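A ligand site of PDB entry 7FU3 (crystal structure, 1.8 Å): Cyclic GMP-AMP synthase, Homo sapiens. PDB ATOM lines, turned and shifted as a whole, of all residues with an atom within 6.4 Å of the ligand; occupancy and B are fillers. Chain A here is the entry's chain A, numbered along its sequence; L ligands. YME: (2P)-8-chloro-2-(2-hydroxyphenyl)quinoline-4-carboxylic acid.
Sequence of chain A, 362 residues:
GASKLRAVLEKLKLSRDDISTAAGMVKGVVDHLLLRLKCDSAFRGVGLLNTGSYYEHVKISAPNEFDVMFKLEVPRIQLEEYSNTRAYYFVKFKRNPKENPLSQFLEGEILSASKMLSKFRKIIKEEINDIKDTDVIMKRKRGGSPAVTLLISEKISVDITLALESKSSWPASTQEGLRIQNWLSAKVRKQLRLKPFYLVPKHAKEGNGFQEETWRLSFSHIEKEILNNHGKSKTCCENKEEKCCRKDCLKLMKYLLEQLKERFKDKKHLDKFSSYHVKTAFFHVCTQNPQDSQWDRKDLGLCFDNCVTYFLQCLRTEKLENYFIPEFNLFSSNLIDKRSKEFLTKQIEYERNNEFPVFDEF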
ATOM      1  N   LYS A  59     -12.151 -15.916   4.701  1.00  0.00           N
ATOM      2  CA  LYS A  59     -10.777 -15.427   4.809  1.00  0.00           C
ATOM      3  C   LYS A  59     -10.772 -13.906   4.728  1.00  0.00           C
ATOM      4  O   LYS A  59     -11.481 -13.307   3.907  1.00  0.00           O
ATOM      5  CB  LYS A  59      -9.912 -16.026   3.697  1.00  0.00           C
ATOM      6  CG  LYS A  59      -8.433 -15.640   3.707  1.00  0.00           C
ATOM      7  CD  LYS A  59      -7.730 -16.289   2.534  1.00  0.00           C
ATOM      8  CE  LYS A  59      -6.272 -15.866   2.428  1.00  0.00           C
ATOM      9  NZ  LYS A  59      -5.599 -16.572   1.294  1.00  0.00           N
ATOM     10  N   SER A  61      -8.161 -10.790   4.036  1.00  0.00           N
ATOM     11  CA  SER A  61      -6.841 -10.444   3.520  1.00  0.00           C
ATOM     12  C   SER A  61      -6.601  -8.942   3.486  1.00  0.00           C
ATOM     13  O   SER A  61      -5.511  -8.524   3.086  1.00  0.00           O
ATOM     14  CB  SER A  61      -6.634 -11.020   2.124  1.00  0.00           C
ATOM     15  OG  SER A  61      -6.501 -12.441   2.144  1.00  0.00           O
ATOM     16  N   ASP A  67     -12.407 -13.068   1.510  1.00  0.00           N
ATOM     17  CA  ASP A  67     -12.095 -14.025   0.462  1.00  0.00           C
ATOM     18  C   ASP A  67     -12.729 -15.357   0.816  1.00  0.00           C
ATOM     19  O   ASP A  67     -12.553 -15.855   1.933  1.00  0.00           O
ATOM     20  CB  ASP A  67     -10.572 -14.214   0.291  1.00  0.00           C
ATOM     21  CG  ASP A  67      -9.863 -12.962  -0.239  1.00  0.00           C
ATOM     22  OD1 ASP A  67     -10.400 -12.317  -1.161  1.00  0.00           O
ATOM     23  OD2 ASP A  67      -8.761 -12.635   0.268  1.00  0.00           O
ATOM     24  N   MET A  69     -13.545 -19.361  -0.993  1.00  0.00           N
ATOM     25  CA  MET A  69     -13.334 -20.302  -2.097  1.00  0.00           C
ATOM     26  C   MET A  69     -14.409 -21.378  -2.096  1.00  0.00           C
ATOM     27  O   MET A  69     -14.734 -21.953  -1.053  1.00  0.00           O
ATOM     28  CB  MET A  69     -11.954 -20.953  -2.007  1.00  0.00           C
ATOM     29  CG  MET A  69     -10.806 -20.012  -2.332  1.00  0.00           C
ATOM     30  SD  MET A  69      -9.235 -20.840  -2.669  1.00  0.00           S
ATOM     31  CE  MET A  69      -9.824 -22.351  -3.392  1.00  0.00           C
ATOM     32  N   ALA A  87       3.107 -23.130 -12.906  1.00  0.00           N
ATOM     33  CA  ALA A  87       1.920 -22.886 -12.109  1.00  0.00           C
ATOM     34  C   ALA A  87       0.604 -22.942 -12.882  1.00  0.00           C
ATOM     35  O   ALA A  87      -0.441 -23.155 -12.260  1.00  0.00           O
ATOM     36  CB  ALA A  87       2.001 -21.534 -11.398  1.00  0.00           C
ATOM     37  N   TYR A  88       0.623 -22.760 -14.189  1.00  0.00           N
ATOM     38  CA  TYR A  88      -0.599 -22.719 -14.984  1.00  0.00           C
ATOM     39  C   TYR A  88      -0.741 -24.003 -15.800  1.00  0.00           C
ATOM     40  O   TYR A  88       0.224 -24.475 -16.402  1.00  0.00           O
ATOM     41  CB  TYR A  88      -0.614 -21.494 -15.889  1.00  0.00           C
ATOM     42  CG  TYR A  88      -0.699 -20.171 -15.128  1.00  0.00           C
ATOM     43  CD1 TYR A  88       0.439 -19.515 -14.686  1.00  0.00           C
ATOM     44  CD2 TYR A  88      -1.932 -19.585 -14.863  1.00  0.00           C
ATOM     45  CE1 TYR A  88       0.360 -18.310 -13.993  1.00  0.00           C
ATOM     46  CE2 TYR A  88      -2.022 -18.388 -14.168  1.00  0.00           C
ATOM     47  CZ  TYR A  88      -0.874 -17.761 -13.738  1.00  0.00           C
ATOM     48  OH  TYR A  88      -0.979 -16.571 -13.054  1.00  0.00           O
ATOM     49  N   VAL A 200      -7.521 -22.910  -9.714  1.00  0.00           N
ATOM     50  CA  VAL A 200      -8.464 -21.803  -9.892  1.00  0.00           C
ATOM     51  C   VAL A 200      -8.325 -21.284 -11.319  1.00  0.00           C
ATOM     52  O   VAL A 200      -7.214 -21.276 -11.877  1.00  0.00           O
ATOM     53  CB  VAL A 200      -8.213 -20.676  -8.873  1.00  0.00           C
ATOM     54  CG1 VAL A 200      -8.097 -21.251  -7.450  1.00  0.00           C
ATOM     55  CG2 VAL A 200      -6.987 -19.908  -9.235  1.00  0.00           C
ATOM     56  N   ARG A 216      -4.724 -22.187 -12.429  1.00  0.00           N
ATOM     57  CA  ARG A 216      -3.560 -21.958 -11.580  1.00  0.00           C
ATOM     58  C   ARG A 216      -3.673 -22.773 -10.304  1.00  0.00           C
ATOM     59  O   ARG A 216      -4.751 -22.890  -9.718  1.00  0.00           O
ATOM     60  CB  ARG A 216      -3.419 -20.476 -11.244  1.00  0.00           C
ATOM     61  CG  ARG A 216      -2.171 -20.190 -10.432  1.00  0.00           C
ATOM     62  CD  ARG A 216      -1.883 -18.709 -10.392  1.00  0.00           C
ATOM     63  NE  ARG A 216      -2.635 -18.026  -9.350  1.00  0.00           N
ATOM     64  CZ  ARG A 216      -2.906 -16.729  -9.363  1.00  0.00           C
ATOM     65  NH1 ARG A 216      -2.478 -15.976 -10.373  1.00  0.00           N
ATOM     66  NH2 ARG A 216      -3.605 -16.185  -8.365  1.00  0.00           N
ATOM     67  N   LEU A 217      -2.545 -23.326  -9.852  1.00  0.00           N
ATOM     68  CA  LEU A 217      -2.535 -24.103  -8.630  1.00  0.00           C
ATOM     69  C   LEU A 217      -2.781 -23.199  -7.426  1.00  0.00           C
ATOM     70  O   LEU A 217      -2.422 -22.022  -7.416  1.00  0.00           O
ATOM     71  CB  LEU A 217      -1.197 -24.819  -8.448  1.00  0.00           C
ATOM     72  CG  LEU A 217      -0.780 -25.823  -9.509  1.00  0.00           C
ATOM     73  CD1 LEU A 217       0.587 -26.359  -9.154  1.00  0.00           C
ATOM     74  CD2 LEU A 217      -1.784 -26.954  -9.645  1.00  0.00           C
ATOM     75  N   SER A 218      -3.399 -23.778  -6.396  1.00  0.00           N
ATOM     76  CA  SER A 218      -3.724 -23.030  -5.186  1.00  0.00           C
ATOM     77  C   SER A 218      -3.551 -23.959  -3.998  1.00  0.00           C
ATOM     78  O   SER A 218      -3.993 -25.102  -4.030  1.00  0.00           O
ATOM     79  CB  SER A 218      -5.159 -22.494  -5.220  1.00  0.00           C
ATOM     80  OG  SER A 218      -5.524 -21.975  -3.951  1.00  0.00           O
ATOM     81  N   PHE A 219      -2.920 -23.441  -2.956  1.00  0.00           N
ATOM     82  CA  PHE A 219      -2.703 -24.263  -1.770  1.00  0.00           C
ATOM     83  C   PHE A 219      -3.132 -23.511  -0.521  1.00  0.00           C
ATOM     84  O   PHE A 219      -2.595 -23.746   0.569  1.00  0.00           O
ATOM     85  CB  PHE A 219      -1.236 -24.688  -1.691  1.00  0.00           C
ATOM     86  CG  PHE A 219      -0.812 -25.542  -2.837  1.00  0.00           C
ATOM     87  CD1 PHE A 219      -0.948 -26.915  -2.774  1.00  0.00           C
ATOM     88  CD2 PHE A 219      -0.280 -24.984  -3.987  1.00  0.00           C
ATOM     89  CE1 PHE A 219      -0.537 -27.710  -3.840  1.00  0.00           C
ATOM     90  CE2 PHE A 219       0.126 -25.770  -5.052  1.00  0.00           C
ATOM     91  CZ  PHE A 219      -0.013 -27.136  -4.973  1.00  0.00           C
ATOM     92  N   SER A 220      -4.107 -22.624  -0.657  1.00  0.00           N
ATOM     93  CA  SER A 220      -4.494 -21.788   0.473  1.00  0.00           C
ATOM     94  C   SER A 220      -5.004 -22.622   1.634  1.00  0.00           C
ATOM     95  O   SER A 220      -4.960 -22.144   2.771  1.00  0.00           O
ATOM     96  CB  SER A 220      -5.541 -20.775   0.057  1.00  0.00           C
ATOM     97  OG  SER A 220      -6.797 -21.408  -0.037  1.00  0.00           O
ATOM     98  N   HIS A 221      -5.450 -23.856   1.393  1.00  0.00           N
ATOM     99  CA  HIS A 221      -5.801 -24.707   2.524  1.00  0.00           C
ATOM    100  C   HIS A 221      -4.563 -25.168   3.292  1.00  0.00           C
ATOM    101  O   HIS A 221      -4.620 -25.307   4.517  1.00  0.00           O
ATOM    102  CB  HIS A 221      -6.613 -25.923   2.055  1.00  0.00           C
ATOM    103  CG  HIS A 221      -5.880 -26.801   1.091  1.00  0.00           C
ATOM    104  ND1 HIS A 221      -5.523 -26.379  -0.167  1.00  0.00           N
ATOM    105  CD2 HIS A 221      -5.429 -28.078   1.195  1.00  0.00           C
ATOM    106  CE1 HIS A 221      -4.878 -27.347  -0.797  1.00  0.00           C
ATOM    107  NE2 HIS A 221      -4.819 -28.392   0.009  1.00  0.00           N
ATOM    108  N   GLU A 223      -1.696 -23.389   3.436  1.00  0.00           N
ATOM    109  CA  GLU A 223      -1.259 -22.174   4.107  1.00  0.00           C
ATOM    110  C   GLU A 223      -1.997 -21.957   5.424  1.00  0.00           C
ATOM    111  O   GLU A 223      -1.375 -21.643   6.454  1.00  0.00           O
ATOM    112  CB  GLU A 223      -1.461 -20.990   3.183  1.00  0.00           C
ATOM    113  CG  GLU A 223      -0.634 -21.170   1.870  1.00  0.00           C
ATOM    114  CD  GLU A 223      -1.080 -20.216   0.760  1.00  0.00           C
ATOM    115  OE1 GLU A 223      -1.874 -19.284   1.037  1.00  0.00           O
ATOM    116  OE2 GLU A 223      -0.633 -20.414  -0.403  1.00  0.00           O
ATOM    117  N   SER A 274       0.741  -7.392  -2.793  1.00  0.00           N
ATOM    118  CA  SER A 274      -0.416  -8.060  -2.221  1.00  0.00           C
ATOM    119  C   SER A 274       0.001  -8.705  -0.916  1.00  0.00           C
ATOM    120  O   SER A 274       1.169  -9.042  -0.733  1.00  0.00           O
ATOM    121  CB  SER A 274      -0.968  -9.122  -3.204  1.00  0.00           C
ATOM    122  OG  SER A 274      -1.710 -10.131  -2.533  1.00  0.00           O
ATOM    123  N   TYR A 276      -0.385 -11.514  -0.222  1.00  0.00           N
ATOM    124  CA  TYR A 276       0.141 -12.831  -0.574  1.00  0.00           C
ATOM    125  C   TYR A 276       1.653 -12.797  -0.720  1.00  0.00           C
ATOM    126  O   TYR A 276       2.329 -13.778  -0.399  1.00  0.00           O
ATOM    127  CB  TYR A 276      -0.491 -13.344  -1.855  1.00  0.00           C
ATOM    128  CG  TYR A 276      -0.120 -14.785  -2.145  1.00  0.00           C
ATOM    129  CD1 TYR A 276      -0.644 -15.824  -1.380  1.00  0.00           C
ATOM    130  CD2 TYR A 276       0.764 -15.105  -3.169  1.00  0.00           C
ATOM    131  CE1 TYR A 276      -0.317 -17.140  -1.643  1.00  0.00           C
ATOM    132  CE2 TYR A 276       1.114 -16.429  -3.438  1.00  0.00           C
ATOM    133  CZ  TYR A 276       0.568 -17.424  -2.658  1.00  0.00           C
ATOM    134  OH  TYR A 276       0.902 -18.737  -2.915  1.00  0.00           O
ATOM    135  N   HIS A 277       2.213 -11.678  -1.189  1.00  0.00           N
ATOM    136  CA  HIS A 277       3.669 -11.552  -1.257  1.00  0.00           C
ATOM    137  C   HIS A 277       4.273 -11.534   0.134  1.00  0.00           C
ATOM    138  O   HIS A 277       5.300 -12.176   0.392  1.00  0.00           O
ATOM    139  CB  HIS A 277       4.037 -10.290  -2.006  1.00  0.00           C
ATOM    140  CG  HIS A 277       3.574 -10.264  -3.426  1.00  0.00           C
ATOM    141  ND1 HIS A 277       2.909  -9.184  -3.975  1.00  0.00           N
ATOM    142  CD2 HIS A 277       3.659 -11.186  -4.405  1.00  0.00           C
ATOM    143  CE1 HIS A 277       2.618  -9.446  -5.236  1.00  0.00           C
ATOM    144  NE2 HIS A 277       3.067 -10.658  -5.527  1.00  0.00           N
ATOM    145  N   ASN A 322       7.454 -18.625  -5.010  1.00  0.00           N
ATOM    146  CA  ASN A 322       6.256 -19.250  -4.483  1.00  0.00           C
ATOM    147  C   ASN A 322       6.653 -20.347  -3.496  1.00  0.00           C
ATOM    148  O   ASN A 322       7.557 -21.138  -3.773  1.00  0.00           O
ATOM    149  CB  ASN A 322       5.435 -19.808  -5.659  1.00  0.00           C
ATOM    150  CG  ASN A 322       4.108 -20.372  -5.252  1.00  0.00           C
ATOM    151  OD1 ASN A 322       4.040 -21.363  -4.530  1.00  0.00           O
ATOM    152  ND2 ASN A 322       3.034 -19.770  -5.750  1.00  0.00           N
ATOM    153  N   PHE A 324       5.275 -22.974  -2.695  1.00  0.00           N
ATOM    154  CA  PHE A 324       4.959 -24.314  -3.162  1.00  0.00           C
ATOM    155  C   PHE A 324       5.553 -24.623  -4.519  1.00  0.00           C
ATOM    156  O   PHE A 324       5.816 -25.791  -4.815  1.00  0.00           O
ATOM    157  CB  PHE A 324       3.430 -24.489  -3.212  1.00  0.00           C
ATOM    158  CG  PHE A 324       2.774 -24.317  -1.880  1.00  0.00           C
ATOM    159  CD1 PHE A 324       2.414 -23.056  -1.424  1.00  0.00           C
ATOM    160  CD2 PHE A 324       2.528 -25.406  -1.065  1.00  0.00           C
ATOM    161  CE1 PHE A 324       1.820 -22.881  -0.185  1.00  0.00           C
ATOM    162  CE2 PHE A 324       1.935 -25.244   0.179  1.00  0.00           C
ATOM    163  CZ  PHE A 324       1.584 -23.973   0.619  1.00  0.00           C
ATOM    164  N   ILE A 325       5.780 -23.607  -5.348  1.00  0.00           N
ATOM    165  CA  ILE A 325       6.367 -23.792  -6.673  1.00  0.00           C
ATOM    166  C   ILE A 325       7.628 -22.943  -6.740  1.00  0.00           C
ATOM    167  O   ILE A 325       7.548 -21.748  -7.072  1.00  0.00           O
ATOM    168  CB  ILE A 325       5.368 -23.395  -7.777  1.00  0.00           C
ATOM    169  CG1 ILE A 325       3.999 -24.055  -7.512  1.00  0.00           C
ATOM    170  CG2 ILE A 325       5.925 -23.765  -9.151  1.00  0.00           C
ATOM    171  CD1 ILE A 325       2.834 -23.160  -7.779  1.00  0.00           C
ATOM    172  N   PHE A 328       8.583 -20.537  -9.649  1.00  0.00           N
ATOM    173  CA  PHE A 328       7.675 -19.448  -9.960  1.00  0.00           C
ATOM    174  C   PHE A 328       8.054 -18.255  -9.103  1.00  0.00           C
ATOM    175  O   PHE A 328       7.775 -18.235  -7.897  1.00  0.00           O
ATOM    176  CB  PHE A 328       6.210 -19.820  -9.726  1.00  0.00           C
ATOM    177  CG  PHE A 328       5.262 -18.878 -10.388  1.00  0.00           C
ATOM    178  CD1 PHE A 328       4.869 -17.732  -9.751  1.00  0.00           C
ATOM    179  CD2 PHE A 328       4.808 -19.128 -11.662  1.00  0.00           C
ATOM    180  CE1 PHE A 328       4.030 -16.832 -10.382  1.00  0.00           C
ATOM    181  CE2 PHE A 328       3.952 -18.253 -12.291  1.00  0.00           C
ATOM    182  CZ  PHE A 328       3.574 -17.099 -11.643  1.00  0.00           C
ATOM    183  N   LEU A 330       7.363 -14.778  -7.861  1.00  0.00           N
ATOM    184  CA  LEU A 330       6.295 -13.792  -7.794  1.00  0.00           C
ATOM    185  C   LEU A 330       6.767 -12.381  -8.121  1.00  0.00           C
ATOM    186  O   LEU A 330       5.944 -11.515  -8.395  1.00  0.00           O
ATOM    187  CB  LEU A 330       5.668 -13.825  -6.404  1.00  0.00           C
ATOM    188  CG  LEU A 330       5.240 -15.195  -5.903  1.00  0.00           C
ATOM    189  CD1 LEU A 330       4.872 -15.101  -4.431  1.00  0.00           C
ATOM    190  CD2 LEU A 330       4.028 -15.614  -6.674  1.00  0.00           C
ATOM    191  N   LEU A 335       5.670  -9.867 -14.045  1.00  0.00           N
ATOM    192  CA  LEU A 335       4.577  -9.612 -13.116  1.00  0.00           C
ATOM    193  C   LEU A 335       4.606  -8.224 -12.500  1.00  0.00           C
ATOM    194  O   LEU A 335       3.547  -7.600 -12.352  1.00  0.00           O
ATOM    195  CB  LEU A 335       4.578 -10.648 -11.991  1.00  0.00           C
ATOM    196  CG  LEU A 335       4.291 -12.076 -12.471  1.00  0.00           C
ATOM    197  CD1 LEU A 335       4.476 -13.065 -11.363  1.00  0.00           C
ATOM    198  CD2 LEU A 335       2.892 -12.188 -13.040  1.00  0.00           C
HETATM  199  C10 YME L   1       0.447 -17.006  -7.653  1.00  0.00           C
HETATM  200  O12 YME L   1      -4.817 -19.531  -3.603  1.00  0.00           O
HETATM  201  O14 YME L   1       0.413 -15.684  -7.427  1.00  0.00           O
HETATM  202  C15 YME L   1      -4.225 -16.646  -3.139  1.00  0.00           C
HETATM  203  C16 YME L   1      -0.100 -19.341  -7.281  1.00  0.00           C
HETATM  204  C17 YME L   1      -4.509 -15.314  -2.971  1.00  0.00           C
HETATM  205  C18 YME L   1      -3.795 -14.315  -3.688  1.00  0.00           C
HETATM  206  C19 YME L   1       1.304 -17.377  -8.696  1.00  0.00           C
HETATM  207  C20 YME L   1       0.746 -19.691  -8.291  1.00  0.00           C
HETATM  208  C21 YME L   1       1.449 -18.700  -9.005  1.00  0.00           C
HETATM  209  C2  YME L   1      -1.260 -17.673  -5.923  1.00  0.00           C
HETATM  210  C3  YME L   1      -2.862 -18.425  -4.318  1.00  0.00           C
HETATM  211  C4  YME L   1      -2.531 -16.072  -4.777  1.00  0.00           C
HETATM  212  C5  YME L   1      -3.231 -17.063  -4.049  1.00  0.00           C
HETATM  213  C6  YME L   1      -1.907 -18.731  -5.233  1.00  0.00           C
HETATM  214  C7  YME L   1      -0.281 -17.988  -6.946  1.00  0.00           C
HETATM  215  C8  YME L   1      -3.463 -19.559  -3.586  1.00  0.00           C
HETATM  216  C9  YME L   1      -2.829 -14.716  -4.540  1.00  0.00           C
HETATM  217  N1  YME L   1      -1.545 -16.376  -5.714  1.00  0.00           N
HETATM  218  O11 YME L   1      -2.864 -20.470  -2.996  1.00  0.00           O
HETATM  219 CL13 YME L   1      -1.843 -13.540  -5.291  1.00  0.00          CL
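The side-chain carboxylate (OE2) of Glu 223 sits close to an oxygen (O11) of the ligand (3.4 Å). Residues that only touch the ligand: Phe 328 (3.3 Å), Asn 322 (3.4 Å), Tyr 276 (3.5 Å), Leu 217 (3.5 Å), Leu 330 (3.7 Å) and Ala 87 (3.8 Å). Hydrophobic or aromatic side chains that line the ligand: Ala 87, Tyr 276, Phe 328 and Leu 330. Of the 23 residues printed, 11 come within 4 Å of the ligand.
The backbone carbonyl oxygen (O) of Phe 328 lies within hydrogen-bond range of the backbone NH (N) of Asn 322 (2.9 Å). The guanidinium group (NH1) of Arg 216 lies within hydrogen-bond range of the side-chain hydroxyl (OH) of Tyr 88. N of Arg 216 sits at hydrogen-bond distance from O of Val 200 (2.7 Å). The side-chain amide oxygen of Asn 322 sits at hydrogen-bond distance from the backbone NH of Ile 325, at 3.0 Å. OD1 of Asn 322 is in hydrogen-bond range of N of Phe 324. The side-chain carboxylate (OE2) of Glu 223 is in hydrogen-bond range of the side-chain hydroxyl (OH) of Tyr 276. OG of Ser 274 lies close to N of Tyr 276, 3.0 Å away. N of Leu 217 is in hydrogen-bond range of O of Ala 87, at 3.2 Å.
The side-chain hydroxyl (OG) of Ser 218 lies within hydrogen-bond range of an oxygen (O12) of the ligand (2.6 Å). N of Phe 219 lies within hydrogen-bond range of O11 of the ligand, 3.0 Å away. The guanidinium group (NH2) of Arg 216 lies within hydrogen-bond range of a nitrogen (N1) of the ligand, 3.4 Å away. The backbone NH of Ser 220 is in hydrogen-bond range of an oxygen (O11) of the ligand (3.4 Å).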
